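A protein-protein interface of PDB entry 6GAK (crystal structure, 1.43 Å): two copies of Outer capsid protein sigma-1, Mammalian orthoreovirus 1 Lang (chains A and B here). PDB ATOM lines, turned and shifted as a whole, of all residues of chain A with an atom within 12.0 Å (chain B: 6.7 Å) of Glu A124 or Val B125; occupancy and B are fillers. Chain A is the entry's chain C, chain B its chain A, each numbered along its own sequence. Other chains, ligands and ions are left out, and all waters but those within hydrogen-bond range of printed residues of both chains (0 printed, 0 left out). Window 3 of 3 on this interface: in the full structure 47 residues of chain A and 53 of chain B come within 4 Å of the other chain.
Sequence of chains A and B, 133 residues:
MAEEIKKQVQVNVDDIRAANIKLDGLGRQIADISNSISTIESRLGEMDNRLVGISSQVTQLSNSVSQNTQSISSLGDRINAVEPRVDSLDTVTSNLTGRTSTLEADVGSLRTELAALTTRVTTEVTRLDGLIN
The side-chain hydroxyl (OG1) of Thr B122 is in hydrogen-bond range of the guanidinium group (NH2) of Arg A120 (2.7 Å). The guanidinium group (NH2) of Arg A127 is in salt-bridge range of the side-chain carboxylate (OD2) of Asp B129, at 2.9 Å.
The side-chain hydroxyl (OG1) of Thr B126 lies within hydrogen-bond range of the backbone carbonyl oxygen (O) of Thr B122, at 3.0 Å. The guanidinium group (NH2) of Arg A127 lies within salt-bridge range of the side-chain carboxylate (OE1) of Glu A124 (2.8 Å).
CZ of Arg A120 touches CG1 of Val B121, 3.8 Å away. CG2 of Val A121 touches CG2 of Val B121 (3.8 Å). Glu A124 touches Val B125. Val B125 touches Arg A127. Leu A128 touches Leu B128 (CD1 to CD1, 3.7 Å). Leu A128 touches Asp B129.
Of the printed residues of chain B, Glu A124 touches Val B125 (3.7 Å). Of chain A, only Glu A124 and Arg A127 come within 4 Å of Val B125. Of the printed residues of chain A, Val B121 touches Arg A120 and Val A121. Thr B122 touches just one residue of chain A: Arg A120 (2.7 Å). Glu B124 touches none of the printed residues of chain A. No residue of chain A comes within 4 Å of Thr B126. Of the printed residues of chain B, Arg A127 touches Val B125 and Asp B129. Printed residues of chain B within 4 Å of Arg A120: Val B121 (3.8 Å) and Thr B122 (2.7 Å). Of the printed residues of chain B, Val A121 touches Val B121 (3.8 Å). Of the printed residues of chain B, Leu A128 touches Leu B128 and Asp B129. Leu A131 touches none of the printed residues of chain B. The nearest residue of chain A that does not touch Val B125 is Leu A128 (4.5 Å). The nearest printed residue of chain B that does not touch Leu A128 is Val B125 (4.5 Å).
Of the 11 printed residues of chain B, 5 touch a printed residue of chain A. Printed residues of chain A that touch a printed residue of chain B: Arg A120, Val A121, Glu A124, Arg A127 and Leu A128. Hydrophobic or aromatic side chains of chain A within 4 Å of the printed part of chain B: Val A121 and Leu A128. Among the printed residues, Asp or Glu carboxylates within 4 Å of a Lys or Arg side-chain nitrogen of the other chain: Arg A127 with Asp B129.
Arg A120 touches Thr B122, but with the chains exchanged Thr A122 does not touch Arg B120 (12.0 Å). Glu A124 touches Val B125, but with the chains exchanged Val A125 does not touch Glu B124 (8.9 Å). Arg A127 touches Asp B129, but with the chains exchanged Asp A129 does not touch Arg B127 (11.9 Å). Leu A128 touches Asp B129, but with the chains exchanged Asp A129 does not touch Leu B128 (8.2 Å). Of the 8 pairs that touch across the chains among the printed residues, 2 have their exchanged pair printed and touching as well.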
ATOM      1  N   ALA A 115     -11.746  -8.173 -13.900  1.00  0.00           N
ATOM      2  CA  ALA A 115     -11.876  -9.423 -13.100  1.00  0.00           C
ATOM      3  C   ALA A 115     -11.594 -10.646 -14.026  1.00  0.00           C
ATOM      4  O   ALA A 115     -10.878 -11.557 -13.626  1.00  0.00           O
ATOM      5  CB  ALA A 115     -13.287  -9.517 -12.541  1.00  0.00           C
ATOM      6  N   ALA A 116     -12.037 -10.591 -15.282  1.00  0.00           N
ATOM      7  CA  ALA A 116     -11.786 -11.716 -16.232  1.00  0.00           C
ATOM      8  C   ALA A 116     -10.249 -11.808 -16.570  1.00  0.00           C
ATOM      9  O   ALA A 116      -9.654 -12.907 -16.683  1.00  0.00           O
ATOM     10  CB  ALA A 116     -12.561 -11.503 -17.521  1.00  0.00           C
ATOM     11  N   LEU A 117      -9.605 -10.628 -16.731  1.00  0.00           N
ATOM     12  CA  LEU A 117      -8.144 -10.616 -16.989  1.00  0.00           C
ATOM     13  C   LEU A 117      -7.383 -11.092 -15.763  1.00  0.00           C
ATOM     14  O   LEU A 117      -6.389 -11.811 -15.928  1.00  0.00           O
ATOM     15  CB  LEU A 117      -7.684  -9.215 -17.362  1.00  0.00           C
ATOM     16  CG  LEU A 117      -6.192  -9.085 -17.793  1.00  0.00           C
ATOM     17  CD1 LEU A 117      -5.932  -9.960 -18.991  1.00  0.00           C
ATOM     18  CD2 LEU A 117      -5.888  -7.640 -18.194  1.00  0.00           C
ATOM     19  N   THR A 118      -7.880 -10.786 -14.550  1.00  0.00           N
ATOM     20  CA  THR A 118      -7.236 -11.287 -13.305  1.00  0.00           C
ATOM     21  C   THR A 118      -7.253 -12.834 -13.293  1.00  0.00           C
ATOM     22  O   THR A 118      -6.222 -13.485 -13.021  1.00  0.00           O
ATOM     23  CB  THR A 118      -7.974 -10.743 -12.099  1.00  0.00           C
ATOM     24  OG1 THR A 118      -7.842  -9.297 -12.104  1.00  0.00           O
ATOM     25  CG2 THR A 118      -7.374 -11.256 -10.797  1.00  0.00           C
ATOM     26  N   THR A 119      -8.411 -13.423 -13.624  1.00  0.00           N
ATOM     27  CA  THR A 119      -8.435 -14.896 -13.666  1.00  0.00           C
ATOM     28  C   THR A 119      -7.650 -15.441 -14.794  1.00  0.00           C
ATOM     29  O   THR A 119      -7.013 -16.482 -14.607  1.00  0.00           O
ATOM     30  CB  THR A 119      -9.805 -15.584 -13.366  1.00  0.00           C
ATOM     31  OG1 THR A 119     -10.160 -16.688 -14.222  1.00  0.00           O
ATOM     32  CG2 THR A 119     -10.874 -14.686 -13.079  1.00  0.00           C
ATOM     33  N   ARG A 120      -7.567 -14.749 -15.936  1.00  0.00           N
ATOM     34  CA  ARG A 120      -6.711 -15.209 -17.040  1.00  0.00           C
ATOM     35  C   ARG A 120      -5.233 -15.235 -16.624  1.00  0.00           C
ATOM     36  O   ARG A 120      -4.527 -16.200 -16.940  1.00  0.00           O
ATOM     37  CB  ARG A 120      -6.888 -14.302 -18.275  1.00  0.00           C
ATOM     38  CG  ARG A 120      -5.918 -14.629 -19.432  1.00  0.00           C
ATOM     39  CD  ARG A 120      -6.192 -13.724 -20.636  1.00  0.00           C
ATOM     40  NE  ARG A 120      -5.219 -14.017 -21.680  1.00  0.00           N
ATOM     41  CZ  ARG A 120      -4.635 -13.121 -22.457  1.00  0.00           C
ATOM     42  NH1 ARG A 120      -4.984 -11.841 -22.385  1.00  0.00           N
ATOM     43  NH2 ARG A 120      -3.711 -13.497 -23.331  1.00  0.00           N
ATOM     44  N   VAL A 121      -4.783 -14.222 -15.860  1.00  0.00           N
ATOM     45  CA  VAL A 121      -3.398 -14.207 -15.385  1.00  0.00           C
ATOM     46  C   VAL A 121      -3.193 -15.411 -14.469  1.00  0.00           C
ATOM     47  O   VAL A 121      -2.198 -16.108 -14.609  1.00  0.00           O
ATOM     48  CB  VAL A 121      -3.067 -12.831 -14.724  1.00  0.00           C
ATOM     49  CG1 VAL A 121      -1.728 -12.901 -13.965  1.00  0.00           C
ATOM     50  CG2 VAL A 121      -3.047 -11.715 -15.783  1.00  0.00           C
ATOM     51  N   THR A 122      -4.144 -15.689 -13.554  1.00  0.00           N
ATOM     52  CA  THR A 122      -3.980 -16.836 -12.643  1.00  0.00           C
ATOM     53  C   THR A 122      -3.919 -18.129 -13.446  1.00  0.00           C
ATOM     54  O   THR A 122      -3.060 -18.981 -13.199  1.00  0.00           O
ATOM     55  CB  THR A 122      -5.154 -16.851 -11.653  1.00  0.00           C
ATOM     56  OG1 THR A 122      -5.077 -15.668 -10.878  1.00  0.00           O
ATOM     57  CG2 THR A 122      -5.134 -18.082 -10.707  1.00  0.00           C
ATOM     58  N   THR A 123      -4.799 -18.289 -14.419  1.00  0.00           N
ATOM     59  CA  THR A 123      -4.825 -19.503 -15.259  1.00  0.00           C
ATOM     60  C   THR A 123      -3.547 -19.716 -16.023  1.00  0.00           C
ATOM     61  O   THR A 123      -2.980 -20.826 -16.037  1.00  0.00           O
ATOM     62  CB  THR A 123      -6.054 -19.396 -16.231  1.00  0.00           C
ATOM     63  OG1 THR A 123      -7.226 -19.467 -15.449  1.00  0.00           O
ATOM     64  CG2 THR A 123      -6.087 -20.534 -17.277  1.00  0.00           C
ATOM     65  N   GLU A 124      -3.066 -18.659 -16.682  1.00  0.00           N
ATOM     66  CA  GLU A 124      -1.860 -18.779 -17.503  1.00  0.00           C
ATOM     67  C   GLU A 124      -0.594 -19.011 -16.647  1.00  0.00           C
ATOM     68  O   GLU A 124       0.251 -19.847 -17.015  1.00  0.00           O
ATOM     69  CB  GLU A 124      -1.697 -17.572 -18.427  1.00  0.00           C
ATOM     70  CG  GLU A 124      -2.809 -17.444 -19.480  1.00  0.00           C
ATOM     71  CD  GLU A 124      -3.043 -18.623 -20.411  1.00  0.00           C
ATOM     72  OE1 GLU A 124      -2.062 -19.308 -20.755  1.00  0.00           O
ATOM     73  OE2 GLU A 124      -4.211 -18.877 -20.782  1.00  0.00           O
ATOM     74  N   VAL A 125      -0.486 -18.349 -15.492  1.00  0.00           N
ATOM     75  CA  VAL A 125       0.677 -18.545 -14.626  1.00  0.00           C
ATOM     76  C   VAL A 125       0.649 -19.973 -14.082  1.00  0.00           C
ATOM     77  O   VAL A 125       1.685 -20.660 -14.086  1.00  0.00           O
ATOM     78  CB  VAL A 125       0.684 -17.495 -13.484  1.00  0.00           C
ATOM     79  CG1 VAL A 125       1.704 -17.883 -12.387  1.00  0.00           C
ATOM     80  CG2 VAL A 125       1.009 -16.109 -14.074  1.00  0.00           C
ATOM     81  N   THR A 126      -0.525 -20.464 -13.691  1.00  0.00           N
ATOM     82  CA  THR A 126      -0.650 -21.867 -13.209  1.00  0.00           C
ATOM     83  C   THR A 126      -0.190 -22.852 -14.309  1.00  0.00           C
ATOM     84  O   THR A 126       0.590 -23.817 -14.031  1.00  0.00           O
ATOM     85  CB  THR A 126      -2.100 -22.162 -12.785  1.00  0.00           C
ATOM     86  OG1 THR A 126      -2.411 -21.385 -11.635  1.00  0.00           O
ATOM     87  CG2 THR A 126      -2.317 -23.653 -12.424  1.00  0.00           C
ATOM     88  N   ARG A 127      -0.673 -22.650 -15.538  1.00  0.00           N
ATOM     89  CA  ARG A 127      -0.314 -23.494 -16.682  1.00  0.00           C
ATOM     90  C   ARG A 127       1.180 -23.472 -16.950  1.00  0.00           C
ATOM     91  O   ARG A 127       1.816 -24.566 -17.075  1.00  0.00           O
ATOM     92  CB  ARG A 127      -1.086 -23.039 -17.944  1.00  0.00           C
ATOM     93  CG  ARG A 127      -0.916 -24.016 -19.137  1.00  0.00           C
ATOM     94  CD  ARG A 127      -1.593 -23.519 -20.407  1.00  0.00           C
ATOM     95  NE  ARG A 127      -1.155 -22.159 -20.766  1.00  0.00           N
ATOM     96  CZ  ARG A 127      -0.046 -21.854 -21.435  1.00  0.00           C
ATOM     97  NH1 ARG A 127       0.781 -22.818 -21.857  1.00  0.00           N
ATOM     98  NH2 ARG A 127       0.257 -20.584 -21.684  1.00  0.00           N
ATOM     99  N   LEU A 128       1.791 -22.263 -17.023  1.00  0.00           N
ATOM    100  CA  LEU A 128       3.241 -22.129 -17.246  1.00  0.00           C
ATOM    101  C   LEU A 128       4.054 -22.786 -16.131  1.00  0.00           C
ATOM    102  O   LEU A 128       5.004 -23.533 -16.451  1.00  0.00           O
ATOM    103  CB  LEU A 128       3.660 -20.659 -17.448  1.00  0.00           C
ATOM    104  CG  LEU A 128       3.083 -20.000 -18.727  1.00  0.00           C
ATOM    105  CD1 LEU A 128       3.220 -18.460 -18.648  1.00  0.00           C
ATOM    106  CD2 LEU A 128       3.740 -20.536 -20.019  1.00  0.00           C
ATOM    107  N   ASP A 129       3.658 -22.607 -14.879  1.00  0.00           N
ATOM    108  CA  ASP A 129       4.322 -23.225 -13.710  1.00  0.00           C
ATOM    109  C   ASP A 129       4.322 -24.769 -13.868  1.00  0.00           C
ATOM    110  O   ASP A 129       5.333 -25.434 -13.568  1.00  0.00           O
ATOM    111  CB  ASP A 129       3.628 -22.844 -12.399  1.00  0.00           C
ATOM    112  CG  ASP A 129       4.284 -21.707 -11.640  1.00  0.00           C
ATOM    113  OD1 ASP A 129       5.545 -21.599 -11.684  1.00  0.00           O
ATOM    114  OD2 ASP A 129       3.552 -20.937 -10.987  1.00  0.00           O
ATOM    115  N   GLY A 130       3.205 -25.314 -14.324  1.00  0.00           N
ATOM    116  CA  GLY A 130       3.043 -26.758 -14.573  1.00  0.00           C
ATOM    117  C   GLY A 130       3.984 -27.297 -15.640  1.00  0.00           C
ATOM    118  O   GLY A 130       4.413 -28.457 -15.554  1.00  0.00           O
ATOM    119  N   LEU A 131       4.337 -26.473 -16.641  1.00  0.00           N
ATOM    120  CA  LEU A 131       5.253 -26.898 -17.703  1.00  0.00           C
ATOM    121  C   LEU A 131       6.732 -26.801 -17.295  1.00  0.00           C
ATOM    122  O   LEU A 131       7.580 -27.470 -17.887  1.00  0.00           O
ATOM    123  CB  LEU A 131       5.031 -26.081 -18.985  1.00  0.00           C
ATOM    124  CG  LEU A 131       3.673 -26.131 -19.682  1.00  0.00           C
ATOM    125  CD1 LEU A 131       3.640 -25.083 -20.776  1.00  0.00           C
ATOM    126  CD2 LEU A 131       3.377 -27.519 -20.256  1.00  0.00           C
ATOM    127  N   ILE A 132       7.057 -25.972 -16.305  1.00  0.00           N
ATOM    128  CA  ILE A 132       8.434 -25.772 -15.823  1.00  0.00           C
ATOM    129  C   ILE A 132       8.737 -26.782 -14.709  1.00  0.00           C
ATOM    130  O   ILE A 132       9.773 -27.419 -14.741  1.00  0.00           O
ATOM    131  CB  ILE A 132       8.630 -24.301 -15.350  1.00  0.00           C
ATOM    132  CG1 ILE A 132       8.388 -23.327 -16.531  1.00  0.00           C
ATOM    133  CG2 ILE A 132      10.009 -24.073 -14.694  1.00  0.00           C
ATOM    134  CD1 ILE A 132       8.016 -21.854 -16.171  1.00  0.00           C
ATOM    135  N   ARG B 120      -0.364  -6.918 -23.168  1.00  0.00           N
ATOM    136  CA  ARG B 120       0.876  -7.309 -22.487  1.00  0.00           C
ATOM    137  C   ARG B 120       0.789  -8.733 -21.945  1.00  0.00           C
ATOM    138  O   ARG B 120       1.758  -9.497 -22.066  1.00  0.00           O
ATOM    139  CB  ARG B 120       1.205  -6.280 -21.397  1.00  0.00           C
ATOM    140  CG  ARG B 120       2.383  -6.659 -20.510  1.00  0.00           C
ATOM    141  CD  ARG B 120       2.603  -5.695 -19.372  1.00  0.00           C
ATOM    142  NE  ARG B 120       3.759  -6.156 -18.607  1.00  0.00           N
ATOM    143  CZ  ARG B 120       3.917  -6.025 -17.292  1.00  0.00           C
ATOM    144  NH1 ARG B 120       2.986  -5.378 -16.552  1.00  0.00           N
ATOM    145  NH2 ARG B 120       4.991  -6.539 -16.701  1.00  0.00           N
ATOM    146  N   VAL B 121      -0.347  -9.113 -21.367  1.00  0.00           N
ATOM    147  CA  VAL B 121      -0.480 -10.482 -20.879  1.00  0.00           C
ATOM    148  C   VAL B 121      -0.374 -11.451 -22.092  1.00  0.00           C
ATOM    149  O   VAL B 121       0.353 -12.433 -22.009  1.00  0.00           O
ATOM    150  CB  VAL B 121      -1.800 -10.648 -20.121  1.00  0.00           C
ATOM    151  CG1 VAL B 121      -2.088 -12.162 -19.844  1.00  0.00           C
ATOM    152  CG2 VAL B 121      -1.785  -9.830 -18.826  1.00  0.00           C
ATOM    153  N   THR B 122      -1.018 -11.131 -23.217  1.00  0.00           N
ATOM    154  CA  THR B 122      -0.889 -12.011 -24.390  1.00  0.00           C
ATOM    155  C   THR B 122       0.550 -12.118 -24.874  1.00  0.00           C
ATOM    156  O   THR B 122       1.045 -13.247 -25.083  1.00  0.00           O
ATOM    157  CB  THR B 122      -1.801 -11.463 -25.495  1.00  0.00           C
ATOM    158  OG1 THR B 122      -3.132 -11.536 -25.065  1.00  0.00           O
ATOM    159  CG2 THR B 122      -1.653 -12.304 -26.833  1.00  0.00           C
ATOM    160  N   THR B 123       1.248 -10.999 -25.032  1.00  0.00           N
ATOM    161  CA  THR B 123       2.647 -10.968 -25.542  1.00  0.00           C
ATOM    162  C   THR B 123       3.587 -11.723 -24.589  1.00  0.00           C
ATOM    163  O   THR B 123       4.448 -12.493 -25.034  1.00  0.00           O
ATOM    164  CB  THR B 123       3.119  -9.484 -25.619  1.00  0.00           C
ATOM    165  OG1 THR B 123       2.239  -8.732 -26.435  1.00  0.00           O
ATOM    166  CG2 THR B 123       4.542  -9.325 -26.132  1.00  0.00           C
ATOM    167  N   GLU B 124       3.460 -11.497 -23.285  1.00  0.00           N
ATOM    168  CA  GLU B 124       4.362 -12.149 -22.312  1.00  0.00           C
ATOM    169  C   GLU B 124       4.089 -13.647 -22.218  1.00  0.00           C
ATOM    170  O   GLU B 124       5.045 -14.425 -22.119  1.00  0.00           O
ATOM    171  CB  GLU B 124       4.256 -11.470 -20.937  1.00  0.00           C
ATOM    172  CG  GLU B 124       4.768 -10.026 -20.959  1.00  0.00           C
ATOM    173  CD  GLU B 124       6.189  -9.756 -21.390  1.00  0.00           C
ATOM    174  OE1 GLU B 124       7.054 -10.603 -21.103  1.00  0.00           O
ATOM    175  OE2 GLU B 124       6.439  -8.698 -22.009  1.00  0.00           O
ATOM    176  N   VAL B 125       2.813 -14.069 -22.267  1.00  0.00           N
ATOM    177  CA  VAL B 125       2.490 -15.503 -22.195  1.00  0.00           C
ATOM    178  C   VAL B 125       3.046 -16.187 -23.467  1.00  0.00           C
ATOM    179  O   VAL B 125       3.674 -17.252 -23.365  1.00  0.00           O
ATOM    180  CB  VAL B 125       0.989 -15.745 -21.991  1.00  0.00           C
ATOM    181  CG1 VAL B 125       0.630 -17.215 -22.255  1.00  0.00           C
ATOM    182  CG2 VAL B 125       0.568 -15.320 -20.569  1.00  0.00           C
ATOM    183  N   THR B 126       2.880 -15.538 -24.628  1.00  0.00           N
ATOM    184  CA  THR B 126       3.414 -16.063 -25.909  1.00  0.00           C
ATOM    185  C   THR B 126       4.904 -16.244 -25.796  1.00  0.00           C
ATOM    186  O   THR B 126       5.421 -17.313 -26.178  1.00  0.00           O
ATOM    187  CB  THR B 126       2.999 -15.135 -27.065  1.00  0.00           C
ATOM    188  OG1 THR B 126       1.570 -15.241 -27.233  1.00  0.00           O
ATOM    189  CG2 THR B 126       3.710 -15.468 -28.392  1.00  0.00           C
ATOM    190  N   ARG B 127       5.614 -15.219 -25.288  1.00  0.00           N
ATOM    191  CA  ARG B 127       7.070 -15.227 -25.147  1.00  0.00           C
ATOM    192  C   ARG B 127       7.506 -16.380 -24.235  1.00  0.00           C
ATOM    193  O   ARG B 127       8.414 -17.164 -24.618  1.00  0.00           O
ATOM    194  CB  ARG B 127       7.573 -13.871 -24.649  1.00  0.00           C
ATOM    195  CG  ARG B 127       9.090 -13.784 -24.571  1.00  0.00           C
ATOM    196  CD  ARG B 127       9.629 -12.502 -23.962  1.00  0.00           C
ATOM    197  NE  ARG B 127       9.077 -12.262 -22.623  1.00  0.00           N
ATOM    198  CZ  ARG B 127       9.531 -12.803 -21.497  1.00  0.00           C
ATOM    199  NH1 ARG B 127      10.563 -13.646 -21.520  1.00  0.00           N
ATOM    200  NH2 ARG B 127       8.923 -12.547 -20.337  1.00  0.00           N
ATOM    201  N   LEU B 128       6.890 -16.503 -23.031  1.00  0.00           N
ATOM    202  CA  LEU B 128       7.217 -17.594 -22.090  1.00  0.00           C
ATOM    203  C   LEU B 128       6.980 -18.971 -22.694  1.00  0.00           C
ATOM    204  O   LEU B 128       7.876 -19.828 -22.603  1.00  0.00           O
ATOM    205  CB  LEU B 128       6.468 -17.396 -20.763  1.00  0.00           C
ATOM    206  CG  LEU B 128       6.873 -16.122 -19.986  1.00  0.00           C
ATOM    207  CD1 LEU B 128       5.838 -15.824 -18.841  1.00  0.00           C
ATOM    208  CD2 LEU B 128       8.269 -16.250 -19.350  1.00  0.00           C
ATOM    209  N   ASP B 129       5.850 -19.158 -23.398  1.00  0.00           N
ATOM    210  CA  ASP B 129       5.503 -20.414 -24.083  1.00  0.00           C
ATOM    211  C   ASP B 129       6.582 -20.806 -25.094  1.00  0.00           C
ATOM    212  O   ASP B 129       6.948 -21.983 -25.169  1.00  0.00           O
ATOM    213  CB  ASP B 129       4.139 -20.307 -24.778  1.00  0.00           C
ATOM    214  CG  ASP B 129       2.976 -20.868 -23.983  1.00  0.00           C
ATOM    215  OD1 ASP B 129       3.158 -21.923 -23.309  1.00  0.00           O
ATOM    216  OD2 ASP B 129       1.860 -20.319 -24.107  1.00  0.00           O
ATOM    217  N   GLY B 130       7.070 -19.820 -25.843  1.00  0.00           N
ATOM    218  CA  GLY B 130       8.133 -19.979 -26.831  1.00  0.00           C
ATOM    219  C   GLY B 130       9.458 -20.433 -26.236  1.00  0.00           C
ATOM    220  O   GLY B 130      10.207 -21.162 -26.904  1.00  0.00           O
